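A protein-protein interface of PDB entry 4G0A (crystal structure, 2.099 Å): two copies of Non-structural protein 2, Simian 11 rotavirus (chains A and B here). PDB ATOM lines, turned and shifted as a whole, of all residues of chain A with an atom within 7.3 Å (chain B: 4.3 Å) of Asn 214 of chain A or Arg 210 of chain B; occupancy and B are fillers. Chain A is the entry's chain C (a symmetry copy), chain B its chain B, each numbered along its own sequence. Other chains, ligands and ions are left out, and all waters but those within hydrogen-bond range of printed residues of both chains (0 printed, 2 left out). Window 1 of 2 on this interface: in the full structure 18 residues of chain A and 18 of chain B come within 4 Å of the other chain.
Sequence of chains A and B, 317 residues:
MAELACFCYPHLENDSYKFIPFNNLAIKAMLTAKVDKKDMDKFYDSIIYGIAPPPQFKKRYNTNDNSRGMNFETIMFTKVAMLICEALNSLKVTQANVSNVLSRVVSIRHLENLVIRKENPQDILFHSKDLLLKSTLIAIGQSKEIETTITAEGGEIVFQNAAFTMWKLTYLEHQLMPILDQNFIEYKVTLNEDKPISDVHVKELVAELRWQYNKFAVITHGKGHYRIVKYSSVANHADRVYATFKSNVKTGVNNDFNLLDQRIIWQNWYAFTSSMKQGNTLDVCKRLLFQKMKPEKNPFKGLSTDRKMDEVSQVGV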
ATOM      1  N   GLU A 208      -1.015  -0.472 -13.882  1.00  0.00           N
ATOM      2  CA  GLU A 208      -1.312  -0.394 -12.454  1.00  0.00           C
ATOM      3  C   GLU A 208      -2.288  -1.489 -12.018  1.00  0.00           C
ATOM      4  O   GLU A 208      -2.110  -2.104 -10.972  1.00  0.00           O
ATOM      5  CB  GLU A 208      -1.868   0.986 -12.094  1.00  0.00           C
ATOM      6  CG  GLU A 208      -2.251   1.144 -10.624  1.00  0.00           C
ATOM      7  CD  GLU A 208      -1.049   1.256  -9.696  1.00  0.00           C
ATOM      8  OE1 GLU A 208       0.103   1.248 -10.186  1.00  0.00           O
ATOM      9  OE2 GLU A 208      -1.259   1.356  -8.469  1.00  0.00           O
ATOM     10  N   LEU A 209      -3.319  -1.723 -12.826  1.00  0.00           N
ATOM     11  CA  LEU A 209      -4.314  -2.748 -12.519  1.00  0.00           C
ATOM     12  C   LEU A 209      -3.708  -4.151 -12.475  1.00  0.00           C
ATOM     13  O   LEU A 209      -3.990  -4.927 -11.561  1.00  0.00           O
ATOM     14  CB  LEU A 209      -5.469  -2.696 -13.519  1.00  0.00           C
ATOM     15  CG  LEU A 209      -6.365  -1.457 -13.413  1.00  0.00           C
ATOM     16  CD1 LEU A 209      -7.371  -1.412 -14.560  1.00  0.00           C
ATOM     17  CD2 LEU A 209      -7.075  -1.429 -12.063  1.00  0.00           C
ATOM     18  N   ARG A 210      -2.872  -4.474 -13.457  1.00  0.00           N
ATOM     19  CA  ARG A 210      -2.235  -5.790 -13.513  1.00  0.00           C
ATOM     20  C   ARG A 210      -1.253  -6.010 -12.368  1.00  0.00           C
ATOM     21  O   ARG A 210      -1.124  -7.120 -11.854  1.00  0.00           O
ATOM     22  CB  ARG A 210      -1.519  -5.987 -14.852  1.00  0.00           C
ATOM     23  CG  ARG A 210      -2.454  -6.083 -16.043  1.00  0.00           C
ATOM     24  CD  ARG A 210      -1.684  -6.323 -17.329  1.00  0.00           C
ATOM     25  NE  ARG A 210      -2.571  -6.412 -18.484  1.00  0.00           N
ATOM     26  CZ  ARG A 210      -2.152  -6.520 -19.740  1.00  0.00           C
ATOM     27  NH1 ARG A 210      -0.852  -6.550 -20.006  1.00  0.00           N
ATOM     28  NH2 ARG A 210      -3.032  -6.595 -20.731  1.00  0.00           N
ATOM     29  N   TRP A 211      -0.559  -4.950 -11.972  1.00  0.00           N
ATOM     30  CA  TRP A 211       0.450  -5.057 -10.930  1.00  0.00           C
ATOM     31  C   TRP A 211      -0.156  -4.989  -9.532  1.00  0.00           C
ATOM     32  O   TRP A 211       0.066  -5.875  -8.703  1.00  0.00           O
ATOM     33  CB  TRP A 211       1.501  -3.958 -11.086  1.00  0.00           C
ATOM     34  CG  TRP A 211       2.476  -3.915  -9.953  1.00  0.00           C
ATOM     35  CD1 TRP A 211       2.469  -3.050  -8.898  1.00  0.00           C
ATOM     36  CD2 TRP A 211       3.595  -4.787  -9.753  1.00  0.00           C
ATOM     37  NE1 TRP A 211       3.520  -3.325  -8.056  1.00  0.00           N
ATOM     38  CE2 TRP A 211       4.227  -4.387  -8.559  1.00  0.00           C
ATOM     39  CE3 TRP A 211       4.125  -5.864 -10.469  1.00  0.00           C
ATOM     40  CZ2 TRP A 211       5.361  -5.027  -8.064  1.00  0.00           C
ATOM     41  CZ3 TRP A 211       5.252  -6.497  -9.977  1.00  0.00           C
ATOM     42  CH2 TRP A 211       5.858  -6.076  -8.787  1.00  0.00           C
ATOM     43  N   GLN A 212      -0.921  -3.933  -9.278  1.00  0.00           N
ATOM     44  CA  GLN A 212      -1.428  -3.659  -7.938  1.00  0.00           C
ATOM     45  C   GLN A 212      -2.759  -4.350  -7.631  1.00  0.00           C
ATOM     46  O   GLN A 212      -3.109  -4.538  -6.467  1.00  0.00           O
ATOM     47  CB  GLN A 212      -1.563  -2.149  -7.721  1.00  0.00           C
ATOM     48  CG  GLN A 212      -1.828  -1.759  -6.279  1.00  0.00           C
ATOM     49  CD  GLN A 212      -0.684  -2.147  -5.366  1.00  0.00           C
ATOM     50  OE1 GLN A 212       0.487  -1.959  -5.705  1.00  0.00           O
ATOM     51  NE2 GLN A 212      -1.013  -2.701  -4.207  1.00  0.00           N
ATOM     52  N   TYR A 213      -3.492  -4.735  -8.671  1.00  0.00           N
ATOM     53  CA  TYR A 213      -4.827  -5.298  -8.485  1.00  0.00           C
ATOM     54  C   TYR A 213      -5.047  -6.545  -9.331  1.00  0.00           C
ATOM     55  O   TYR A 213      -6.092  -6.702  -9.960  1.00  0.00           O
ATOM     56  CB  TYR A 213      -5.883  -4.239  -8.809  1.00  0.00           C
ATOM     57  CG  TYR A 213      -5.667  -2.966  -8.027  1.00  0.00           C
ATOM     58  CD1 TYR A 213      -6.185  -2.822  -6.748  1.00  0.00           C
ATOM     59  CD2 TYR A 213      -4.917  -1.923  -8.553  1.00  0.00           C
ATOM     60  CE1 TYR A 213      -5.975  -1.666  -6.018  1.00  0.00           C
ATOM     61  CE2 TYR A 213      -4.702  -0.760  -7.835  1.00  0.00           C
ATOM     62  CZ  TYR A 213      -5.237  -0.640  -6.563  1.00  0.00           C
ATOM     63  OH  TYR A 213      -5.030   0.509  -5.836  1.00  0.00           O
ATOM     64  N   ASN A 214      -4.059  -7.434  -9.334  1.00  0.00           N
ATOM     65  CA  ASN A 214      -4.094  -8.616 -10.192  1.00  0.00           C
ATOM     66  C   ASN A 214      -5.216  -9.587  -9.850  1.00  0.00           C
ATOM     67  O   ASN A 214      -5.641 -10.368 -10.700  1.00  0.00           O
ATOM     68  CB  ASN A 214      -2.747  -9.348 -10.167  1.00  0.00           C
ATOM     69  CG  ASN A 214      -2.528 -10.117  -8.877  1.00  0.00           C
ATOM     70  OD1 ASN A 214      -2.473  -9.533  -7.796  1.00  0.00           O
ATOM     71  ND2 ASN A 214      -2.389 -11.434  -8.988  1.00  0.00           N
ATOM     72  N   LYS A 215      -5.693  -9.544  -8.609  1.00  0.00           N
ATOM     73  CA  LYS A 215      -6.762 -10.438  -8.177  1.00  0.00           C
ATOM     74  C   LYS A 215      -8.149  -9.843  -8.413  1.00  0.00           C
ATOM     75  O   LYS A 215      -9.153 -10.367  -7.927  1.00  0.00           O
ATOM     76  CB  LYS A 215      -6.594 -10.819  -6.700  1.00  0.00           C
ATOM     77  CG  LYS A 215      -5.340 -11.637  -6.409  1.00  0.00           C
ATOM     78  CD  LYS A 215      -5.385 -12.247  -5.014  1.00  0.00           C
ATOM     79  CE  LYS A 215      -5.365 -11.177  -3.941  1.00  0.00           C
ATOM     80  NZ  LYS A 215      -4.107 -10.385  -3.996  1.00  0.00           N
ATOM     81  N   PHE A 216      -8.206  -8.749  -9.161  1.00  0.00           N
ATOM     82  CA  PHE A 216      -9.473  -8.068  -9.400  1.00  0.00           C
ATOM     83  C   PHE A 216      -9.818  -8.049 -10.879  1.00  0.00           C
ATOM     84  O   PHE A 216      -8.954  -7.814 -11.725  1.00  0.00           O
ATOM     85  CB  PHE A 216      -9.427  -6.642  -8.846  1.00  0.00           C
ATOM     86  CG  PHE A 216      -9.366  -6.579  -7.345  1.00  0.00           C
ATOM     87  CD1 PHE A 216      -8.172  -6.799  -6.676  1.00  0.00           C
ATOM     88  CD2 PHE A 216     -10.504  -6.311  -6.601  1.00  0.00           C
ATOM     89  CE1 PHE A 216      -8.114  -6.747  -5.290  1.00  0.00           C
ATOM     90  CE2 PHE A 216     -10.454  -6.259  -5.217  1.00  0.00           C
ATOM     91  CZ  PHE A 216      -9.254  -6.477  -4.561  1.00  0.00           C
ATOM     92  N   ALA A 217     -11.089  -8.304 -11.180  1.00  0.00           N
ATOM     93  CA  ALA A 217     -11.597  -8.213 -12.540  1.00  0.00           C
ATOM     94  C   ALA A 217     -11.947  -6.768 -12.874  1.00  0.00           C
ATOM     95  O   ALA A 217     -12.443  -6.024 -12.026  1.00  0.00           O
ATOM     96  CB  ALA A 217     -12.825  -9.105 -12.705  1.00  0.00           C
ATOM     97  N   TYR A 231     -12.645 -11.340  -8.507  1.00  0.00           N
ATOM     98  CA  TYR A 231     -13.116 -12.336  -9.459  1.00  0.00           C
ATOM     99  C   TYR A 231     -14.216 -13.194  -8.848  1.00  0.00           C
ATOM    100  O   TYR A 231     -15.110 -13.667  -9.548  1.00  0.00           O
ATOM    101  CB  TYR A 231     -11.959 -13.205  -9.950  1.00  0.00           C
ATOM    102  CG  TYR A 231     -11.128 -12.533 -11.010  1.00  0.00           C
ATOM    103  CD1 TYR A 231     -11.565 -12.485 -12.328  1.00  0.00           C
ATOM    104  CD2 TYR A 231      -9.914 -11.931 -10.697  1.00  0.00           C
ATOM    105  CE1 TYR A 231     -10.814 -11.867 -13.305  1.00  0.00           C
ATOM    106  CE2 TYR A 231      -9.158 -11.309 -11.673  1.00  0.00           C
ATOM    107  CZ  TYR A 231      -9.611 -11.282 -12.971  1.00  0.00           C
ATOM    108  OH  TYR A 231      -8.869 -10.663 -13.950  1.00  0.00           O
ATOM    109  N   VAL B 206       3.959 -22.445  -7.822  1.00  0.00           N
ATOM    110  CA  VAL B 206       4.109 -21.315  -8.733  1.00  0.00           C
ATOM    111  C   VAL B 206       2.780 -20.603  -8.961  1.00  0.00           C
ATOM    112  O   VAL B 206       2.729 -19.374  -9.024  1.00  0.00           O
ATOM    113  CB  VAL B 206       4.712 -21.751 -10.089  1.00  0.00           C
ATOM    114  CG1 VAL B 206       4.677 -20.597 -11.089  1.00  0.00           C
ATOM    115  CG2 VAL B 206       6.133 -22.253  -9.897  1.00  0.00           C
ATOM    116  N   ALA B 207       1.704 -21.375  -9.075  1.00  0.00           N
ATOM    117  CA  ALA B 207       0.377 -20.800  -9.269  1.00  0.00           C
ATOM    118  C   ALA B 207      -0.032 -19.935  -8.073  1.00  0.00           C
ATOM    119  O   ALA B 207      -0.591 -18.847  -8.236  1.00  0.00           O
ATOM    120  CB  ALA B 207      -0.652 -21.896  -9.514  1.00  0.00           C
ATOM    121  N   GLU B 208       0.254 -20.421  -6.870  1.00  0.00           N
ATOM    122  CA  GLU B 208      -0.060 -19.668  -5.660  1.00  0.00           C
ATOM    123  C   GLU B 208       0.783 -18.396  -5.582  1.00  0.00           C
ATOM    124  O   GLU B 208       0.276 -17.327  -5.254  1.00  0.00           O
ATOM    125  CB  GLU B 208       0.146 -20.529  -4.409  1.00  0.00           C
ATOM    126  CG  GLU B 208      -0.144 -19.803  -3.097  1.00  0.00           C
ATOM    127  CD  GLU B 208      -1.619 -19.489  -2.912  1.00  0.00           C
ATOM    128  OE1 GLU B 208      -2.435 -19.949  -3.740  1.00  0.00           O
ATOM    129  OE2 GLU B 208      -1.964 -18.785  -1.938  1.00  0.00           O
ATOM    130  N   LEU B 209       2.070 -18.517  -5.898  1.00  0.00           N
ATOM    131  CA  LEU B 209       2.973 -17.370  -5.855  1.00  0.00           C
ATOM    132  C   LEU B 209       2.602 -16.290  -6.874  1.00  0.00           C
ATOM    133  O   LEU B 209       2.652 -15.097  -6.569  1.00  0.00           O
ATOM    134  CB  LEU B 209       4.424 -17.821  -6.058  1.00  0.00           C
ATOM    135  CG  LEU B 209       5.016 -18.627  -4.893  1.00  0.00           C
ATOM    136  CD1 LEU B 209       6.373 -19.222  -5.262  1.00  0.00           C
ATOM    137  CD2 LEU B 209       5.123 -17.752  -3.653  1.00  0.00           C
ATOM    138  N   ARG B 210       2.223 -16.705  -8.079  1.00  0.00           N
ATOM    139  CA  ARG B 210       1.845 -15.751  -9.121  1.00  0.00           C
ATOM    140  C   ARG B 210       0.522 -15.056  -8.824  1.00  0.00           C
ATOM    141  O   ARG B 210       0.324 -13.901  -9.191  1.00  0.00           O
ATOM    142  CB  ARG B 210       1.765 -16.438 -10.486  1.00  0.00           C
ATOM    143  CG  ARG B 210       3.107 -16.806 -11.082  1.00  0.00           C
ATOM    144  CD  ARG B 210       2.934 -17.472 -12.442  1.00  0.00           C
ATOM    145  NE  ARG B 210       4.202 -17.960 -12.975  1.00  0.00           N
ATOM    146  CZ  ARG B 210       4.314 -18.709 -14.067  1.00  0.00           C
ATOM    147  NH1 ARG B 210       3.230 -19.061 -14.747  1.00  0.00           N
ATOM    148  NH2 ARG B 210       5.510 -19.110 -14.477  1.00  0.00           N
ATOM    149  N   TRP B 211      -0.385 -15.764  -8.162  1.00  0.00           N
ATOM    150  CA  TRP B 211      -1.702 -15.210  -7.870  1.00  0.00           C
ATOM    151  C   TRP B 211      -1.717 -14.377  -6.589  1.00  0.00           C
ATOM    152  O   TRP B 211      -2.136 -13.218  -6.596  1.00  0.00           O
ATOM    153  CB  TRP B 211      -2.743 -16.325  -7.778  1.00  0.00           C
ATOM    154  CG  TRP B 211      -4.098 -15.854  -7.357  1.00  0.00           C
ATOM    155  CD1 TRP B 211      -4.646 -15.941  -6.109  1.00  0.00           C
ATOM    156  CD2 TRP B 211      -5.079 -15.217  -8.184  1.00  0.00           C
ATOM    157  NE1 TRP B 211      -5.910 -15.399  -6.109  1.00  0.00           N
ATOM    158  CE2 TRP B 211      -6.198 -14.949  -7.373  1.00  0.00           C
ATOM    159  CE3 TRP B 211      -5.119 -14.851  -9.531  1.00  0.00           C
ATOM    160  CZ2 TRP B 211      -7.344 -14.330  -7.864  1.00  0.00           C
ATOM    161  CZ3 TRP B 211      -6.259 -14.235 -10.018  1.00  0.00           C
ATOM    162  CH2 TRP B 211      -7.354 -13.982  -9.188  1.00  0.00           C
ATOM    163  N   GLN B 212      -1.254 -14.971  -5.494  1.00  0.00           N
ATOM    164  CA  GLN B 212      -1.357 -14.336  -4.183  1.00  0.00           C
ATOM    165  C   GLN B 212      -0.159 -13.452  -3.842  1.00  0.00           C
ATOM    166  O   GLN B 212      -0.260 -12.583  -2.978  1.00  0.00           O
ATOM    167  CB  GLN B 212      -1.540 -15.396  -3.093  1.00  0.00           C
ATOM    168  CG  GLN B 212      -1.942 -14.823  -1.742  1.00  0.00           C
ATOM    169  CD  GLN B 212      -3.304 -14.160  -1.786  1.00  0.00           C
ATOM    170  OE1 GLN B 212      -4.224 -14.653  -2.437  1.00  0.00           O
ATOM    171  NE2 GLN B 212      -3.435 -13.029  -1.103  1.00  0.00           N
ATOM    172  N   ASN B 214       2.094 -11.820  -6.336  1.00  0.00           N
ATOM    173  CA  ASN B 214       2.614 -11.334  -7.608  1.00  0.00           C
ATOM    174  C   ASN B 214       3.592 -10.167  -7.449  1.00  0.00           C
ATOM    175  O   ASN B 214       4.435  -9.934  -8.314  1.00  0.00           O
ATOM    176  CB  ASN B 214       1.470 -10.960  -8.556  1.00  0.00           C
ATOM    177  CG  ASN B 214       0.924  -9.571  -8.294  1.00  0.00           C
ATOM    178  OD1 ASN B 214       0.352  -9.305  -7.240  1.00  0.00           O
ATOM    179  ND2 ASN B 214       1.090  -8.680  -9.263  1.00  0.00           N
ATOM    180  N   ASN B 298       8.008 -20.048 -20.698  1.00  0.00           N
ATOM    181  CA  ASN B 298       7.141 -20.261 -19.547  1.00  0.00           C
ATOM    182  C   ASN B 298       6.834 -21.743 -19.356  1.00  0.00           C
ATOM    183  O   ASN B 298       6.131 -22.346 -20.167  1.00  0.00           O
ATOM    184  CB  ASN B 298       5.842 -19.468 -19.703  1.00  0.00           C
ATOM    185  CG  ASN B 298       5.014 -19.446 -18.430  1.00  0.00           C
ATOM    186  OD1 ASN B 298       5.227 -20.249 -17.521  1.00  0.00           O
ATOM    187  ND2 ASN B 298       4.059 -18.525 -18.364  1.00  0.00           N
ATOM    188  N   PHE B 300       4.973 -23.196 -17.224  1.00  0.00           N
ATOM    189  CA  PHE B 300       3.568 -23.432 -16.916  1.00  0.00           C
ATOM    190  C   PHE B 300       2.699 -22.272 -17.386  1.00  0.00           C
ATOM    191  O   PHE B 300       2.294 -21.430 -16.583  1.00  0.00           O
ATOM    192  CB  PHE B 300       3.369 -23.616 -15.409  1.00  0.00           C
ATOM    193  CG  PHE B 300       4.455 -24.405 -14.740  1.00  0.00           C
ATOM    194  CD1 PHE B 300       4.505 -25.783 -14.859  1.00  0.00           C
ATOM    195  CD2 PHE B 300       5.416 -23.767 -13.972  1.00  0.00           C
ATOM    196  CE1 PHE B 300       5.501 -26.511 -14.235  1.00  0.00           C
ATOM    197  CE2 PHE B 300       6.412 -24.489 -13.345  1.00  0.00           C
ATOM    198  CZ  PHE B 300       6.456 -25.862 -13.478  1.00  0.00           C
ATOM    199  N   LEU B 303      -1.391 -20.580 -15.855  1.00  0.00           N
ATOM    200  CA  LEU B 303      -1.643 -20.793 -14.432  1.00  0.00           C
ATOM    201  C   LEU B 303      -2.531 -19.702 -13.849  1.00  0.00           C
ATOM    202  O   LEU B 303      -3.442 -19.981 -13.068  1.00  0.00           O
ATOM    203  CB  LEU B 303      -0.332 -20.880 -13.646  1.00  0.00           C
ATOM    204  CG  LEU B 303       0.391 -22.226 -13.723  1.00  0.00           C
ATOM    205  CD1 LEU B 303       1.530 -22.276 -12.720  1.00  0.00           C
ATOM    206  CD2 LEU B 303      -0.588 -23.363 -13.479  1.00  0.00           C
ATOM    207  N   LYS B 308      -8.056 -17.610 -11.969  1.00  0.00           N
ATOM    208  CA  LYS B 308      -9.118 -16.656 -12.252  1.00  0.00           C
ATOM    209  C   LYS B 308     -10.442 -17.382 -12.437  1.00  0.00           C
ATOM    210  O   LYS B 308     -11.443 -17.042 -11.805  1.00  0.00           O
ATOM    211  CB  LYS B 308      -8.804 -15.845 -13.509  1.00  0.00           C
ATOM    212  CG  LYS B 308      -7.876 -14.664 -13.293  1.00  0.00           C
ATOM    213  CD  LYS B 308      -7.673 -13.902 -14.595  1.00  0.00           C
ATOM    214  CE  LYS B 308      -6.779 -12.687 -14.402  1.00  0.00           C
ATOM    215  NZ  LYS B 308      -5.433 -13.038 -13.868  1.00  0.00           N
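The backbone carbonyl oxygen of Trp 211 of chain B sits at hydrogen-bond distance from the side-chain amide nitrogen of Asn 214 of chain A (3.0 Å).
The side-chain amide oxygen (OD1) of Asn 214 of chain B lies close to the side-chain amide oxygen (OD1) of Asn 214 of chain A, 2.9 Å away.
O of Trp 211 of chain A lies within hydrogen-bond range of ND2 of Asn 214 of chain B.
The backbone NH (N) of Asn 214 of chain B is in hydrogen-bond range of the backbone carbonyl oxygen (O) of Leu 209 of chain B, 3.3 Å away.
O of Phe 300 of chain B sits at hydrogen-bond distance from NH1 of Arg 210 of chain B (3.1 Å).
N of Asn 214 of chain A sits at hydrogen-bond distance from O of Leu 209 of chain A.
The guanidinium group of Arg 210 of chain B is in hydrogen-bond range of the side-chain amide oxygen of Asn 298 of chain B, 3.3 Å away.
Among the printed residues, merely in contact across the chains: Tyr 231 of chain A with Lys 308 of chain B (2.9 Å), Lys 215 of chain A with Trp 211 of chain B (3.4 Å), Tyr 231 of chain A with Trp 211 of chain B (3.6 Å), Asn 214 of chain A with Arg 210 of chain B (3.7 Å), Lys 215 of chain A with Gln 212 of chain B (3.7 Å) and Arg 210 of chain A with Asn 214 of chain B (3.7 Å).
Of chain B, only Arg 210, Trp 211 and Asn 214 come within 4 Å of Asn 214 of chain A.
Arg 210 of chain B touches just one residue of chain A: Asn 214 (3.7 Å).
Of the printed residues of chain B, Tyr 231 of chain A touches Trp 211 (3.6 Å) and Lys 308 (2.9 Å).
Of the printed residues of chain A, Trp 211 of chain B touches Asn 214, Lys 215 and Tyr 231.
Of the printed residues of chain B, Arg 210 of chain A touches Asn 214.
The nearest residue of chain A that does not touch Arg 210 of chain B is Lys 215 of chain A (6.7 Å).
Hydrophobic or aromatic side chains of chain A that line the printed part of chain B: Trp 211 and Tyr 231.
Arg 210 of chain A touches Asn 214 of chain B, and with the chains exchanged Asn 214 of chain A touches Arg 210 of chain B.
Trp 211 of chain A touches Asn 214 of chain B, and with the chains exchanged Asn 214 of chain A touches Trp 211 of chain B.
Asn 214 of chain B touches its own counterpart, Asn 214 of chain A.
Positions printed for both chains: 208, 209, 210, 211, 212 and 214.
Of the 9 pairs that touch across the chains among the printed residues, 5 have their exchanged pair printed and touching as well.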
